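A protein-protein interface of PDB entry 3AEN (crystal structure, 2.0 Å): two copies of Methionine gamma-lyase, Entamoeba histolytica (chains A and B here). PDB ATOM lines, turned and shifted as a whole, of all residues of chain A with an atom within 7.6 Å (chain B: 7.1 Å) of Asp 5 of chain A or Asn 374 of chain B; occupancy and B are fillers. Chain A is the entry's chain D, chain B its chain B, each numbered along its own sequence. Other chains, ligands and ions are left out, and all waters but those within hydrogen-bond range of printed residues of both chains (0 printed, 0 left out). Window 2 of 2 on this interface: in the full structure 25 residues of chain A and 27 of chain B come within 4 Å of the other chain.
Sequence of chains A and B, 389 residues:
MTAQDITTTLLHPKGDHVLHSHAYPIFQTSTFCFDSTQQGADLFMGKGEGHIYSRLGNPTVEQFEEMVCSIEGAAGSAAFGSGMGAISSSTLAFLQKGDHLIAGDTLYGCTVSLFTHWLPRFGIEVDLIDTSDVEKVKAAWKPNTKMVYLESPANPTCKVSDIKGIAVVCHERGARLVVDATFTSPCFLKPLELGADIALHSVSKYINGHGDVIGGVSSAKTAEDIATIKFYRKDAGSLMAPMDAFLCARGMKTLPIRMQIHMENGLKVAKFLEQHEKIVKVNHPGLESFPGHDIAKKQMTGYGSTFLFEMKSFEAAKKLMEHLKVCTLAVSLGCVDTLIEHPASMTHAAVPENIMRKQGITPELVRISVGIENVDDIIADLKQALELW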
ATOM      1  N   ASP A   5      11.990  17.949  -2.157  1.00  0.00           N
ATOM      2  CA  ASP A   5      11.929  18.522  -0.784  1.00  0.00           C
ATOM      3  C   ASP A   5      10.518  18.470  -0.160  1.00  0.00           C
ATOM      4  O   ASP A   5       9.529  18.028  -0.792  1.00  0.00           O
ATOM      5  CB  ASP A   5      12.514  19.958  -0.759  1.00  0.00           C
ATOM      6  CG  ASP A   5      11.529  21.044  -1.295  1.00  0.00           C
ATOM      7  OD1 ASP A   5      11.940  22.228  -1.348  1.00  0.00           O
ATOM      8  OD2 ASP A   5      10.368  20.743  -1.668  1.00  0.00           O
ATOM      9  N   ILE A   6      10.451  18.961   1.077  1.00  0.00           N
ATOM     10  CA  ILE A   6       9.275  18.887   1.936  1.00  0.00           C
ATOM     11  C   ILE A   6       8.024  19.623   1.410  1.00  0.00           C
ATOM     12  O   ILE A   6       6.892  19.208   1.705  1.00  0.00           O
ATOM     13  CB  ILE A   6       9.628  19.385   3.359  1.00  0.00           C
ATOM     14  CG1 ILE A   6      11.003  18.834   3.776  1.00  0.00           C
ATOM     15  CG2 ILE A   6       8.547  18.978   4.346  1.00  0.00           C
ATOM     16  CD1 ILE A   6      11.647  19.471   5.050  1.00  0.00           C
ATOM     17  N   THR A   7       8.215  20.692   0.633  1.00  0.00           N
ATOM     18  CA  THR A   7       7.071  21.487   0.170  1.00  0.00           C
ATOM     19  C   THR A   7       6.091  20.646  -0.651  1.00  0.00           C
ATOM     20  O   THR A   7       4.878  20.704  -0.417  1.00  0.00           O
ATOM     21  CB  THR A   7       7.481  22.761  -0.615  1.00  0.00           C
ATOM     22  OG1 THR A   7       8.297  23.596   0.211  1.00  0.00           O
ATOM     23  CG2 THR A   7       6.251  23.548  -1.014  1.00  0.00           C
ATOM     24  N   THR A   8       6.627  19.846  -1.579  1.00  0.00           N
ATOM     25  CA  THR A   8       5.802  18.987  -2.437  1.00  0.00           C
ATOM     26  C   THR A   8       4.922  18.015  -1.635  1.00  0.00           C
ATOM     27  O   THR A   8       3.772  17.795  -2.003  1.00  0.00           O
ATOM     28  CB  THR A   8       6.657  18.197  -3.467  1.00  0.00           C
ATOM     29  OG1 THR A   8       7.502  19.104  -4.187  1.00  0.00           O
ATOM     30  CG2 THR A   8       5.770  17.471  -4.453  1.00  0.00           C
ATOM     31  N   THR A   9       5.462  17.452  -0.551  1.00  0.00           N
ATOM     32  CA  THR A   9       4.746  16.479   0.279  1.00  0.00           C
ATOM     33  C   THR A   9       3.573  17.145   1.006  1.00  0.00           C
ATOM     34  O   THR A   9       2.460  16.595   1.038  1.00  0.00           O
ATOM     35  CB  THR A   9       5.695  15.782   1.323  1.00  0.00           C
ATOM     36  OG1 THR A   9       6.801  15.155   0.654  1.00  0.00           O
ATOM     37  CG2 THR A   9       4.946  14.729   2.110  1.00  0.00           C
ATOM     38  N   LEU A  10       3.823  18.322   1.583  1.00  0.00           N
ATOM     39  CA  LEU A  10       2.787  19.078   2.297  1.00  0.00           C
ATOM     40  C   LEU A  10       1.658  19.552   1.363  1.00  0.00           C
ATOM     41  O   LEU A  10       0.484  19.548   1.753  1.00  0.00           O
ATOM     42  CB  LEU A  10       3.410  20.253   3.076  1.00  0.00           C
ATOM     43  CG  LEU A  10       4.442  19.832   4.128  1.00  0.00           C
ATOM     44  CD1 LEU A  10       5.298  21.008   4.577  1.00  0.00           C
ATOM     45  CD2 LEU A  10       3.790  19.150   5.328  1.00  0.00           C
ATOM     46  N   LEU A  11       2.006  19.904   0.123  1.00  0.00           N
ATOM     47  CA  LEU A  11       1.002  20.348  -0.871  1.00  0.00           C
ATOM     48  C   LEU A  11       0.255  19.183  -1.538  1.00  0.00           C
ATOM     49  O   LEU A  11      -0.795  19.386  -2.150  1.00  0.00           O
ATOM     50  CB  LEU A  11       1.641  21.229  -1.949  1.00  0.00           C
ATOM     51  CG  LEU A  11       2.332  22.515  -1.494  1.00  0.00           C
ATOM     52  CD1 LEU A  11       2.925  23.226  -2.679  1.00  0.00           C
ATOM     53  CD2 LEU A  11       1.363  23.403  -0.798  1.00  0.00           C
ATOM     54  N   ILE A  71       5.969  14.401   7.790  1.00  0.00           N
ATOM     55  CA  ILE A  71       7.201  15.188   8.019  1.00  0.00           C
ATOM     56  C   ILE A  71       8.064  14.693   9.224  1.00  0.00           C
ATOM     57  O   ILE A  71       9.301  14.789   9.186  1.00  0.00           O
ATOM     58  CB  ILE A  71       6.871  16.724   8.072  1.00  0.00           C
ATOM     59  CG1 ILE A  71       8.111  17.598   8.215  1.00  0.00           C
ATOM     60  CG2 ILE A  71       6.036  17.051   9.231  1.00  0.00           C
ATOM     61  CD1 ILE A  71       9.102  17.478   7.118  1.00  0.00           C
ATOM     62  N   PRO A 256       7.870  25.068   4.959  1.00  0.00           N
ATOM     63  CA  PRO A 256       9.299  24.945   4.603  1.00  0.00           C
ATOM     64  C   PRO A 256       9.909  26.258   4.113  1.00  0.00           C
ATOM     65  O   PRO A 256      11.063  26.558   4.383  1.00  0.00           O
ATOM     66  CB  PRO A 256       9.288  23.907   3.469  1.00  0.00           C
ATOM     67  CG  PRO A 256       8.054  23.102   3.740  1.00  0.00           C
ATOM     68  CD  PRO A 256       7.047  24.099   4.210  1.00  0.00           C
ATOM     69  N   ILE A 257       9.105  27.029   3.408  1.00  0.00           N
ATOM     70  CA  ILE A 257       9.495  28.315   2.856  1.00  0.00           C
ATOM     71  C   ILE A 257       9.643  29.411   3.943  1.00  0.00           C
ATOM     72  O   ILE A 257      10.617  30.178   3.916  1.00  0.00           O
ATOM     73  CB  ILE A 257       8.484  28.667   1.738  1.00  0.00           C
ATOM     74  CG1 ILE A 257       8.807  27.822   0.499  1.00  0.00           C
ATOM     75  CG2 ILE A 257       8.461  30.155   1.418  1.00  0.00           C
ATOM     76  CD1 ILE A 257       7.574  27.285  -0.215  1.00  0.00           C
ATOM     77  N   GLN A 260      12.822  28.571   6.044  1.00  0.00           N
ATOM     78  CA  GLN A 260      14.037  29.014   5.353  1.00  0.00           C
ATOM     79  C   GLN A 260      14.342  30.493   5.679  1.00  0.00           C
ATOM     80  O   GLN A 260      15.489  30.845   5.983  1.00  0.00           O
ATOM     81  CB  GLN A 260      13.892  28.805   3.840  1.00  0.00           C
ATOM     82  CG  GLN A 260      15.205  28.586   3.052  1.00  0.00           C
ATOM     83  CD  GLN A 260      14.986  28.686   1.518  1.00  0.00           C
ATOM     84  OE1 GLN A 260      13.886  28.417   1.012  1.00  0.00           O
ATOM     85  NE2 GLN A 260      16.028  29.080   0.790  1.00  0.00           N
ATOM     86  N   ILE B 261       8.796  32.515  -5.722  1.00  0.00           N
ATOM     87  CA  ILE B 261       8.877  31.102  -6.076  1.00  0.00           C
ATOM     88  C   ILE B 261       8.055  30.763  -7.333  1.00  0.00           C
ATOM     89  O   ILE B 261       8.566  30.084  -8.246  1.00  0.00           O
ATOM     90  CB  ILE B 261       8.491  30.176  -4.896  1.00  0.00           C
ATOM     91  CG1 ILE B 261       9.387  30.453  -3.683  1.00  0.00           C
ATOM     92  CG2 ILE B 261       8.636  28.710  -5.312  1.00  0.00           C
ATOM     93  CD1 ILE B 261       8.865  29.833  -2.421  1.00  0.00           C
ATOM     94  N   ASN B 265       9.813  29.211 -10.488  1.00  0.00           N
ATOM     95  CA  ASN B 265       9.270  27.897 -10.853  1.00  0.00           C
ATOM     96  C   ASN B 265       8.689  27.880 -12.263  1.00  0.00           C
ATOM     97  O   ASN B 265       9.102  27.055 -13.075  1.00  0.00           O
ATOM     98  CB  ASN B 265       8.218  27.423  -9.858  1.00  0.00           C
ATOM     99  CG  ASN B 265       8.806  26.721  -8.644  1.00  0.00           C
ATOM    100  OD1 ASN B 265       8.071  26.090  -7.879  1.00  0.00           O
ATOM    101  ND2 ASN B 265      10.105  26.822  -8.457  1.00  0.00           N
ATOM    102  N   VAL B 326       1.333  14.701  -9.951  1.00  0.00           N
ATOM    103  CA  VAL B 326       1.508  15.825  -9.017  1.00  0.00           C
ATOM    104  C   VAL B 326       0.557  16.959  -9.395  1.00  0.00           C
ATOM    105  O   VAL B 326      -0.283  17.357  -8.591  1.00  0.00           O
ATOM    106  CB  VAL B 326       2.986  16.327  -8.967  1.00  0.00           C
ATOM    107  CG1 VAL B 326       3.137  17.508  -8.026  1.00  0.00           C
ATOM    108  CG2 VAL B 326       3.955  15.188  -8.592  1.00  0.00           C
ATOM    109  N   GLY B 371       2.854  25.876  -9.385  1.00  0.00           N
ATOM    110  CA  GLY B 371       2.760  26.181  -7.958  1.00  0.00           C
ATOM    111  C   GLY B 371       4.140  26.375  -7.354  1.00  0.00           C
ATOM    112  O   GLY B 371       5.122  26.565  -8.073  1.00  0.00           O
ATOM    113  N   ILE B 372       4.202  26.301  -6.029  1.00  0.00           N
ATOM    114  CA  ILE B 372       5.436  26.510  -5.278  1.00  0.00           C
ATOM    115  C   ILE B 372       6.057  25.191  -4.775  1.00  0.00           C
ATOM    116  O   ILE B 372       6.899  25.198  -3.874  1.00  0.00           O
ATOM    117  CB  ILE B 372       5.230  27.526  -4.110  1.00  0.00           C
ATOM    118  CG1 ILE B 372       4.210  27.004  -3.082  1.00  0.00           C
ATOM    119  CG2 ILE B 372       4.738  28.882  -4.653  1.00  0.00           C
ATOM    120  CD1 ILE B 372       4.227  27.761  -1.739  1.00  0.00           C
ATOM    121  N   GLU B 373       5.651  24.067  -5.370  1.00  0.00           N
ATOM    122  CA  GLU B 373       6.331  22.781  -5.145  1.00  0.00           C
ATOM    123  C   GLU B 373       7.781  22.926  -5.559  1.00  0.00           C
ATOM    124  O   GLU B 373       8.125  23.876  -6.262  1.00  0.00           O
ATOM    125  CB  GLU B 373       5.719  21.655  -5.985  1.00  0.00           C
ATOM    126  CG  GLU B 373       4.289  21.294  -5.661  1.00  0.00           C
ATOM    127  CD  GLU B 373       3.287  21.950  -6.612  1.00  0.00           C
ATOM    128  OE1 GLU B 373       2.162  21.421  -6.742  1.00  0.00           O
ATOM    129  OE2 GLU B 373       3.623  22.976  -7.238  1.00  0.00           O
ATOM    130  N   ASN B 374       8.628  21.994  -5.119  1.00  0.00           N
ATOM    131  CA  ASN B 374       9.976  21.867  -5.673  1.00  0.00           C
ATOM    132  C   ASN B 374       9.791  21.733  -7.173  1.00  0.00           C
ATOM    133  O   ASN B 374       9.068  20.856  -7.639  1.00  0.00           O
ATOM    134  CB  ASN B 374      10.675  20.626  -5.111  1.00  0.00           C
ATOM    135  CG  ASN B 374      12.104  20.425  -5.661  1.00  0.00           C
ATOM    136  OD1 ASN B 374      12.426  20.781  -6.791  1.00  0.00           O
ATOM    137  ND2 ASN B 374      12.946  19.808  -4.855  1.00  0.00           N
ATOM    138  N   VAL B 375      10.418  22.629  -7.930  1.00  0.00           N
ATOM    139  CA  VAL B 375      10.256  22.654  -9.384  1.00  0.00           C
ATOM    140  C   VAL B 375      10.658  21.310 -10.040  1.00  0.00           C
ATOM    141  O   VAL B 375      10.089  20.909 -11.056  1.00  0.00           O
ATOM    142  CB  VAL B 375      11.020  23.858 -10.006  1.00  0.00           C
ATOM    143  CG1 VAL B 375      12.519  23.700  -9.835  1.00  0.00           C
ATOM    144  CG2 VAL B 375      10.665  24.042 -11.481  1.00  0.00           C
ATOM    145  N   ASP B 376      11.625  20.611  -9.447  1.00  0.00           N
ATOM    146  CA  ASP B 376      12.062  19.312  -9.970  1.00  0.00           C
ATOM    147  C   ASP B 376      10.974  18.251  -9.946  1.00  0.00           C
ATOM    148  O   ASP B 376      10.943  17.395 -10.818  1.00  0.00           O
ATOM    149  CB  ASP B 376      13.282  18.822  -9.216  1.00  0.00           C
ATOM    150  CG  ASP B 376      14.483  19.717  -9.424  1.00  0.00           C
ATOM    151  OD1 ASP B 376      15.343  19.760  -8.525  1.00  0.00           O
ATOM    152  OD2 ASP B 376      14.562  20.382 -10.480  1.00  0.00           O
ATOM    153  N   ASP B 377      10.068  18.319  -8.970  1.00  0.00           N
ATOM    154  CA  ASP B 377       8.951  17.382  -8.917  1.00  0.00           C
ATOM    155  C   ASP B 377       7.935  17.668 -10.006  1.00  0.00           C
ATOM    156  O   ASP B 377       7.322  16.744 -10.530  1.00  0.00           O
ATOM    157  CB  ASP B 377       8.262  17.407  -7.557  1.00  0.00           C
ATOM    158  CG  ASP B 377       9.156  16.949  -6.449  1.00  0.00           C
ATOM    159  OD1 ASP B 377       9.918  15.977  -6.662  1.00  0.00           O
ATOM    160  OD2 ASP B 377       9.099  17.548  -5.359  1.00  0.00           O
ATOM    161  N   ILE B 378       7.737  18.949 -10.315  1.00  0.00           N
ATOM    162  CA  ILE B 378       6.844  19.367 -11.402  1.00  0.00           C
ATOM    163  C   ILE B 378       7.419  18.961 -12.769  1.00  0.00           C
ATOM    164  O   ILE B 378       6.721  18.371 -13.597  1.00  0.00           O
ATOM    165  CB  ILE B 378       6.540  20.898 -11.337  1.00  0.00           C
ATOM    166  CG1 ILE B 378       5.892  21.253  -9.981  1.00  0.00           C
ATOM    167  CG2 ILE B 378       5.599  21.327 -12.474  1.00  0.00           C
ATOM    168  CD1 ILE B 378       6.263  22.651  -9.458  1.00  0.00           C
ATOM    169  N   ILE B 379       8.693  19.272 -12.994  1.00  0.00           N
ATOM    170  CA  ILE B 379       9.373  18.888 -14.225  1.00  0.00           C
ATOM    171  C   ILE B 379       9.350  17.355 -14.411  1.00  0.00           C
ATOM    172  O   ILE B 379       9.038  16.873 -15.501  1.00  0.00           O
ATOM    173  CB  ILE B 379      10.810  19.493 -14.295  1.00  0.00           C
ATOM    174  CG1 ILE B 379      10.713  21.008 -14.524  1.00  0.00           C
ATOM    175  CG2 ILE B 379      11.682  18.794 -15.382  1.00  0.00           C
ATOM    176  CD1 ILE B 379      12.023  21.762 -14.352  1.00  0.00           C
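OD1 of Asn 374 of chain B sits at hydrogen-bond distance from N of Asp 376 of chain B, at 2.8 Å. The side-chain carboxylate (OD2) of Asp 5 of chain A lies within hydrogen-bond range of the backbone NH (N) of Thr 7 of chain A, at 3.2 Å. The side-chain amide oxygen (OD1) of Asn 265 of chain B lies close to the backbone carbonyl oxygen (O) of Glu 373 of chain B (2.7 Å).
ND2 of Asn 374 of chain B sits close to N of Asp 5 of chain A, 3.4 Å away. OD2 of Asp 377 of chain B is in hydrogen-bond range of OG1 of Thr 8 of chain A, 2.5 Å away. N of Asn 374 of chain B is in hydrogen-bond range of OG1 of Thr 8 of chain A.
No position is printed for both chains.
Of the 12 printed residues of chain B, 5 touch a printed residue of chain A. Of the 11 printed residues of chain A, 5 touch a printed residue of chain B. Hydrophobic or aromatic side chains of chain A that line the printed part of chain B: Leu 11 and Ile 257. Among the printed residues, 8 pairs touch across the chains. Among the printed residues, no Asp or Glu carboxylate lies within 4 Å of a Lys or Arg side-chain nitrogen of the other chain.
Of the printed residues of chain B, Leu 11 of chain A touches Glu 373. Pro 256 of chain A touches none of the printed residues of chain B. Printed residues of chain A within 4 Å of Ile 261 of chain B: Ile 257. Of the printed residues of chain A, Ile 372 of chain B touches Thr 7 (3.4 Å) and Ile 257 (3.7 Å). Asn 374 of chain B touches two residues of chain A. Of the printed residues of chain A, Asp 377 of chain B touches Thr 8 (2.5 Å). The nearest residue of chain B that does not touch Asp 5 of chain A is Asp 377 of chain B (4.3 Å). The nearest printed residue of chain B that does not touch Thr 7 of chain A is Glu 373 of chain B (4.2 Å).
Among the printed residues, merely in contact across the chains: Thr 7 of chain A with Ile 372 of chain B (3.4 Å), Ile 257 of chain A with Ile 261 of chain B (3.5 Å), Thr 8 of chain A with Glu 373 of chain B (3.6 Å), Ile 257 of chain A with Ile 372 of chain B (3.7 Å) and Leu 11 of chain A with Glu 373 of chain B (3.8 Å).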
